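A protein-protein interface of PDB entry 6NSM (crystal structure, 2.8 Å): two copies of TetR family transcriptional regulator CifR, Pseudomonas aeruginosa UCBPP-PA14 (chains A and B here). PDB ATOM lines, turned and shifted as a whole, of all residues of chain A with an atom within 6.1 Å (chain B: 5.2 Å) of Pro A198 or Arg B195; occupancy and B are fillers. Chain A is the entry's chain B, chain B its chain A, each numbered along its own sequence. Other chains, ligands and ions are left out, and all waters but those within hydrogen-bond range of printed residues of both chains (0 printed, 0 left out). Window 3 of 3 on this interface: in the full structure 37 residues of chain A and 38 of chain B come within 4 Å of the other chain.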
ATOM      1  N   ARG A  86      32.697  -2.388   8.273  1.00  0.00           N
ATOM      2  CA  ARG A  86      31.702  -2.307   9.337  1.00  0.00           C
ATOM      3  C   ARG A  86      32.296  -1.705  10.604  1.00  0.00           C
ATOM      4  O   ARG A  86      31.648  -0.892  11.273  1.00  0.00           O
ATOM      5  CB  ARG A  86      31.114  -3.688   9.620  1.00  0.00           C
ATOM      6  CG  ARG A  86      29.877  -3.663  10.505  1.00  0.00           C
ATOM      7  CD  ARG A  86      29.606  -5.030  11.104  1.00  0.00           C
ATOM      8  NE  ARG A  86      28.405  -5.049  11.932  1.00  0.00           N
ATOM      9  CZ  ARG A  86      27.305  -5.730  11.642  1.00  0.00           C
ATOM     10  NH1 ARG A  86      27.222  -6.482  10.555  1.00  0.00           N
ATOM     11  NH2 ARG A  86      26.264  -5.664  12.467  1.00  0.00           N
ATOM     12  N   LEU A 153      32.855  -7.243   2.895  1.00  0.00           N
ATOM     13  CA  LEU A 153      31.548  -6.779   2.455  1.00  0.00           C
ATOM     14  C   LEU A 153      31.206  -7.453   1.135  1.00  0.00           C
ATOM     15  O   LEU A 153      32.060  -7.571   0.252  1.00  0.00           O
ATOM     16  CB  LEU A 153      31.540  -5.255   2.280  1.00  0.00           C
ATOM     17  CG  LEU A 153      30.178  -4.572   2.148  1.00  0.00           C
ATOM     18  CD1 LEU A 153      29.269  -4.957   3.301  1.00  0.00           C
ATOM     19  CD2 LEU A 153      30.347  -3.063   2.082  1.00  0.00           C
ATOM     20  N   THR A 157      26.698  -5.520  -2.796  1.00  0.00           N
ATOM     21  CA  THR A 157      26.159  -4.598  -1.842  1.00  0.00           C
ATOM     22  C   THR A 157      25.845  -3.300  -2.524  1.00  0.00           C
ATOM     23  O   THR A 157      26.596  -2.839  -3.349  1.00  0.00           O
ATOM     24  CB  THR A 157      27.154  -4.373  -0.708  1.00  0.00           C
ATOM     25  OG1 THR A 157      27.271  -5.572   0.036  1.00  0.00           O
ATOM     26  CG2 THR A 157      26.676  -3.334   0.220  1.00  0.00           C
ATOM     27  N   LEU A 162      23.847   1.930   1.383  1.00  0.00           N
ATOM     28  CA  LEU A 162      24.462   1.786   2.699  1.00  0.00           C
ATOM     29  C   LEU A 162      25.144   3.077   3.135  1.00  0.00           C
ATOM     30  O   LEU A 162      25.010   3.499   4.289  1.00  0.00           O
ATOM     31  CB  LEU A 162      25.454   0.625   2.683  1.00  0.00           C
ATOM     32  CG  LEU A 162      25.744  -0.064   4.017  1.00  0.00           C
ATOM     33  CD1 LEU A 162      24.456  -0.335   4.781  1.00  0.00           C
ATOM     34  CD2 LEU A 162      26.521  -1.349   3.792  1.00  0.00           C
ATOM     35  N   TYR A 166      23.792   5.531   6.433  1.00  0.00           N
ATOM     36  CA  TYR A 166      24.610   5.914   7.578  1.00  0.00           C
ATOM     37  C   TYR A 166      24.909   7.406   7.576  1.00  0.00           C
ATOM     38  O   TYR A 166      25.129   7.994   8.641  1.00  0.00           O
ATOM     39  CB  TYR A 166      25.890   5.080   7.614  1.00  0.00           C
ATOM     40  CG  TYR A 166      25.657   3.674   8.112  1.00  0.00           C
ATOM     41  CD1 TYR A 166      25.237   3.441   9.415  1.00  0.00           C
ATOM     42  CD2 TYR A 166      25.826   2.581   7.273  1.00  0.00           C
ATOM     43  CE1 TYR A 166      25.009   2.158   9.875  1.00  0.00           C
ATOM     44  CE2 TYR A 166      25.599   1.296   7.723  1.00  0.00           C
ATOM     45  CZ  TYR A 166      25.191   1.090   9.024  1.00  0.00           C
ATOM     46  OH  TYR A 166      24.965  -0.189   9.479  1.00  0.00           O
ATOM     47  N   LEU A 194      23.751  -0.042  13.451  1.00  0.00           N
ATOM     48  CA  LEU A 194      24.648  -1.060  12.961  1.00  0.00           C
ATOM     49  C   LEU A 194      23.967  -2.389  12.772  1.00  0.00           C
ATOM     50  O   LEU A 194      24.433  -3.213  12.035  1.00  0.00           O
ATOM     51  CB  LEU A 194      25.828  -1.207  13.885  1.00  0.00           C
ATOM     52  CG  LEU A 194      26.855  -0.120  13.670  1.00  0.00           C
ATOM     53  CD1 LEU A 194      27.848  -0.116  14.801  1.00  0.00           C
ATOM     54  CD2 LEU A 194      27.555  -0.359  12.361  1.00  0.00           C
ATOM     55  N   ARG A 195      22.849  -2.596  13.436  1.00  0.00           N
ATOM     56  CA  ARG A 195      22.064  -3.802  13.202  1.00  0.00           C
ATOM     57  C   ARG A 195      21.535  -3.870  11.775  1.00  0.00           C
ATOM     58  O   ARG A 195      21.255  -4.966  11.278  1.00  0.00           O
ATOM     59  CB  ARG A 195      20.908  -3.859  14.205  1.00  0.00           C
ATOM     60  CG  ARG A 195      20.111  -5.152  14.198  1.00  0.00           C
ATOM     61  CD  ARG A 195      19.060  -5.142  15.300  1.00  0.00           C
ATOM     62  NE  ARG A 195      17.893  -5.953  14.971  1.00  0.00           N
ATOM     63  CZ  ARG A 195      17.878  -7.279  14.946  1.00  0.00           C
ATOM     64  NH1 ARG A 195      18.961  -7.989  15.215  1.00  0.00           N
ATOM     65  NH2 ARG A 195      16.747  -7.909  14.643  1.00  0.00           N
ATOM     66  N   ALA A 196      21.408  -2.727  11.101  1.00  0.00           N
ATOM     67  CA  ALA A 196      20.977  -2.693   9.710  1.00  0.00           C
ATOM     68  C   ALA A 196      22.071  -3.096   8.730  1.00  0.00           C
ATOM     69  O   ALA A 196      21.787  -3.214   7.532  1.00  0.00           O
ATOM     70  CB  ALA A 196      20.459  -1.297   9.355  1.00  0.00           C
ATOM     71  N   TRP A 197      23.300  -3.293   9.196  1.00  0.00           N
ATOM     72  CA  TRP A 197      24.376  -3.708   8.309  1.00  0.00           C
ATOM     73  C   TRP A 197      24.014  -5.032   7.638  1.00  0.00           C
ATOM     74  O   TRP A 197      23.393  -5.898   8.267  1.00  0.00           O
ATOM     75  CB  TRP A 197      25.673  -3.870   9.104  1.00  0.00           C
ATOM     76  CG  TRP A 197      26.906  -3.932   8.254  1.00  0.00           C
ATOM     77  CD1 TRP A 197      27.506  -5.052   7.760  1.00  0.00           C
ATOM     78  CD2 TRP A 197      27.686  -2.822   7.793  1.00  0.00           C
ATOM     79  NE1 TRP A 197      28.613  -4.710   7.022  1.00  0.00           N
ATOM     80  CE2 TRP A 197      28.745  -3.346   7.026  1.00  0.00           C
ATOM     81  CE3 TRP A 197      27.592  -1.437   7.955  1.00  0.00           C
ATOM     82  CZ2 TRP A 197      29.703  -2.534   6.422  1.00  0.00           C
ATOM     83  CZ3 TRP A 197      28.545  -0.632   7.355  1.00  0.00           C
ATOM     84  CH2 TRP A 197      29.586  -1.183   6.598  1.00  0.00           C
ATOM     85  N   PRO A 198      24.373  -5.222   6.357  1.00  0.00           N
ATOM     86  CA  PRO A 198      24.073  -6.468   5.638  1.00  0.00           C
ATOM     87  C   PRO A 198      24.746  -7.684   6.266  1.00  0.00           C
ATOM     88  O   PRO A 198      25.717  -7.559   7.012  1.00  0.00           O
ATOM     89  CB  PRO A 198      24.624  -6.222   4.228  1.00  0.00           C
ATOM     90  CG  PRO A 198      25.455  -4.996   4.308  1.00  0.00           C
ATOM     91  CD  PRO A 198      25.020  -4.216   5.500  1.00  0.00           C
ATOM     92  OXT PRO A 198      24.331  -8.822   6.041  1.00  0.00           O
ATOM     93  N   ARG B  86       5.706  -1.990  13.779  1.00  0.00           N
ATOM     94  CA  ARG B  86       6.702  -1.952  12.714  1.00  0.00           C
ATOM     95  C   ARG B  86       6.118  -1.372  11.432  1.00  0.00           C
ATOM     96  O   ARG B  86       6.788  -0.608  10.727  1.00  0.00           O
ATOM     97  CB  ARG B  86       7.251  -3.358  12.467  1.00  0.00           C
ATOM     98  CG  ARG B  86       8.469  -3.412  11.555  1.00  0.00           C
ATOM     99  CD  ARG B  86       8.711  -4.826  11.044  1.00  0.00           C
ATOM    100  NE  ARG B  86       9.948  -4.936  10.278  1.00  0.00           N
ATOM    101  CZ  ARG B  86      11.033  -5.578  10.692  1.00  0.00           C
ATOM    102  NH1 ARG B  86      11.062  -6.209  11.853  1.00  0.00           N
ATOM    103  NH2 ARG B  86      12.112  -5.594   9.916  1.00  0.00           N
ATOM    104  N   TYR B 166      14.736   5.992  15.243  1.00  0.00           N
ATOM    105  CA  TYR B 166      13.952   6.303  14.054  1.00  0.00           C
ATOM    106  C   TYR B 166      13.691   7.798  13.930  1.00  0.00           C
ATOM    107  O   TYR B 166      13.532   8.307  12.815  1.00  0.00           O
ATOM    108  CB  TYR B 166      12.649   5.505  14.056  1.00  0.00           C
ATOM    109  CG  TYR B 166      12.841   4.068  13.638  1.00  0.00           C
ATOM    110  CD1 TYR B 166      13.181   3.747  12.330  1.00  0.00           C
ATOM    111  CD2 TYR B 166      12.704   3.032  14.552  1.00  0.00           C
ATOM    112  CE1 TYR B 166      13.365   2.434  11.941  1.00  0.00           C
ATOM    113  CE2 TYR B 166      12.889   1.715  14.173  1.00  0.00           C
ATOM    114  CZ  TYR B 166      13.218   1.421  12.866  1.00  0.00           C
ATOM    115  OH  TYR B 166      13.404   0.113  12.481  1.00  0.00           O
ATOM    116  N   GLU B 191      14.002   1.603   3.918  1.00  0.00           N
ATOM    117  CA  GLU B 191      14.032   0.145   3.967  1.00  0.00           C
ATOM    118  C   GLU B 191      15.211  -0.351   4.797  1.00  0.00           C
ATOM    119  O   GLU B 191      15.064  -1.264   5.616  1.00  0.00           O
ATOM    120  CB  GLU B 191      14.103  -0.422   2.549  1.00  0.00           C
ATOM    121  CG  GLU B 191      12.751  -0.717   1.921  1.00  0.00           C
ATOM    122  CD  GLU B 191      11.710  -1.134   2.940  1.00  0.00           C
ATOM    123  OE1 GLU B 191      11.794  -2.274   3.446  1.00  0.00           O
ATOM    124  OE2 GLU B 191      10.804  -0.325   3.230  1.00  0.00           O
ATOM    125  N   ARG B 192      16.392   0.239   4.591  1.00  0.00           N
ATOM    126  CA  ARG B 192      17.571  -0.164   5.349  1.00  0.00           C
ATOM    127  C   ARG B 192      17.384   0.093   6.840  1.00  0.00           C
ATOM    128  O   ARG B 192      17.778  -0.729   7.674  1.00  0.00           O
ATOM    129  CB  ARG B 192      18.802   0.574   4.822  1.00  0.00           C
ATOM    130  CG  ARG B 192      20.049   0.419   5.679  1.00  0.00           C
ATOM    131  CD  ARG B 192      20.644  -0.975   5.581  1.00  0.00           C
ATOM    132  NE  ARG B 192      20.755  -1.430   4.202  1.00  0.00           N
ATOM    133  CZ  ARG B 192      20.952  -2.693   3.843  1.00  0.00           C
ATOM    134  NH1 ARG B 192      21.116  -3.649   4.743  1.00  0.00           N
ATOM    135  NH2 ARG B 192      20.999  -3.000   2.549  1.00  0.00           N
ATOM    136  N   ALA B 193      16.782   1.233   7.193  1.00  0.00           N
ATOM    137  CA  ALA B 193      16.574   1.559   8.601  1.00  0.00           C
ATOM    138  C   ALA B 193      15.648   0.554   9.270  1.00  0.00           C
ATOM    139  O   ALA B 193      15.840   0.202  10.441  1.00  0.00           O
ATOM    140  CB  ALA B 193      16.018   2.977   8.734  1.00  0.00           C
ATOM    141  N   LEU B 194      14.635   0.079   8.544  1.00  0.00           N
ATOM    142  CA  LEU B 194      13.693  -0.883   9.101  1.00  0.00           C
ATOM    143  C   LEU B 194      14.322  -2.251   9.317  1.00  0.00           C
ATOM    144  O   LEU B 194      13.756  -3.073  10.046  1.00  0.00           O
ATOM    145  CB  LEU B 194      12.472  -1.000   8.194  1.00  0.00           C
ATOM    146  CG  LEU B 194      11.586   0.244   8.198  1.00  0.00           C
ATOM    147  CD1 LEU B 194      10.890   0.398   6.857  1.00  0.00           C
ATOM    148  CD2 LEU B 194      10.588   0.186   9.344  1.00  0.00           C
ATOM    149  N   ARG B 195      15.472  -2.515   8.694  1.00  0.00           N
ATOM    150  CA  ARG B 195      16.196  -3.754   8.943  1.00  0.00           C
ATOM    151  C   ARG B 195      16.807  -3.783  10.340  1.00  0.00           C
ATOM    152  O   ARG B 195      17.115  -4.867  10.849  1.00  0.00           O
ATOM    153  CB  ARG B 195      17.278  -3.924   7.871  1.00  0.00           C
ATOM    154  CG  ARG B 195      18.148  -5.164   8.002  1.00  0.00           C
ATOM    155  CD  ARG B 195      19.182  -5.218   6.887  1.00  0.00           C
ATOM    156  NE  ARG B 195      20.310  -6.080   7.222  1.00  0.00           N
ATOM    157  CZ  ARG B 195      20.291  -7.403   7.144  1.00  0.00           C
ATOM    158  NH1 ARG B 195      19.218  -8.057   6.729  1.00  0.00           N
ATOM    159  NH2 ARG B 195      21.379  -8.089   7.487  1.00  0.00           N
ATOM    160  N   ALA B 196      16.956  -2.627  10.983  1.00  0.00           N
ATOM    161  CA  ALA B 196      17.439  -2.566  12.356  1.00  0.00           C
ATOM    162  C   ALA B 196      16.360  -2.868  13.387  1.00  0.00           C
ATOM    163  O   ALA B 196      16.672  -2.915  14.582  1.00  0.00           O
ATOM    164  CB  ALA B 196      18.053  -1.192  12.639  1.00  0.00           C
ATOM    165  N   TRP B 197      15.115  -3.061  12.961  1.00  0.00           N
ATOM    166  CA  TRP B 197      14.036  -3.325  13.901  1.00  0.00           C
ATOM    167  C   TRP B 197      14.359  -4.577  14.715  1.00  0.00           C
ATOM    168  O   TRP B 197      14.912  -5.543  14.174  1.00  0.00           O
ATOM    169  CB  TRP B 197      12.729  -3.531  13.131  1.00  0.00           C
ATOM    170  CG  TRP B 197      11.503  -3.548  13.993  1.00  0.00           C
ATOM    171  CD1 TRP B 197      10.903  -4.643  14.544  1.00  0.00           C
ATOM    172  CD2 TRP B 197      10.723  -2.418  14.398  1.00  0.00           C
ATOM    173  NE1 TRP B 197       9.800  -4.263  15.268  1.00  0.00           N
ATOM    174  CE2 TRP B 197       9.667  -2.902  15.195  1.00  0.00           C
ATOM    175  CE3 TRP B 197      10.816  -1.042  14.164  1.00  0.00           C
ATOM    176  CZ2 TRP B 197       8.711  -2.059  15.760  1.00  0.00           C
ATOM    177  CZ3 TRP B 197       9.866  -0.208  14.726  1.00  0.00           C
ATOM    178  CH2 TRP B 197       8.827  -0.720  15.514  1.00  0.00           C
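Of the 10 printed residues of chain A, 5 touch a printed residue of chain B.
Along chain A the printed residues that touch a printed residue of chain B span positions 162 to 198.
Hydrophobic or aromatic side chains of chain B that line the printed part of chain A: Ala B196.
The guanidinium group (NH1) of Arg B192 lies within hydrogen-bond range of the backbone carbonyl oxygen (O) of Ala A196, at 2.9 Å.
NE of Arg B195 lies within hydrogen-bond range of O of Ala A196, at 3.2 Å.
NH2 of Arg B195 lies within hydrogen-bond range of O of Trp A197, 3.1 Å away.
NH2 of Arg B195 lies within salt-bridge range of OXT of Pro A198 (3.4 Å).
NE of Arg A195 lies within hydrogen-bond range of O of Ala B196, at 3.3 Å.
The backbone carbonyl oxygen of Trp B197 is in hydrogen-bond range of the guanidinium group of Arg A195 (3.0 Å).
Among the printed residues, pairs that only touch across the chains: Leu A162 with Arg B192 (3.9 Å), Ala A196 with Ala B196 (3.997 Å) and Pro A198 with Arg B192 (3.96 Å).
The chain-end carboxylate (O) of Pro A198 is in salt-bridge range of the guanidinium group (NH1) of Arg A86 (3.997 Å).
Arg A195 touches Ala B196, and with the chains exchanged Ala A196 touches Arg B195.
Arg A195 touches Trp B197, and with the chains exchanged Trp A197 touches Arg B195.
Ala A196 touches its own counterpart, Ala B196.
6 positions are printed for both chains.
Of the 9 pairs that touch across the chains among the printed residues, 5 have their exchanged pair printed and touching as well.
Pro A198 touches just these residues of chain B: Arg B192 (3.96 Å) and Arg B195 (3.4 Å).
Of chain A, only Ala A196, Trp A197 and Pro A198 come within 4 Å of Arg B195.
Of the printed residues of chain A, Trp B197 touches Arg A195 (3.0 Å).
Of the printed residues of chain B, Leu A162 touches Arg B192 (3.9 Å).
Tyr B166 touches none of the printed residues of chain A.
The nearest printed residue of chain B that does not touch Trp A197 is Arg B192 (4.3 Å).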
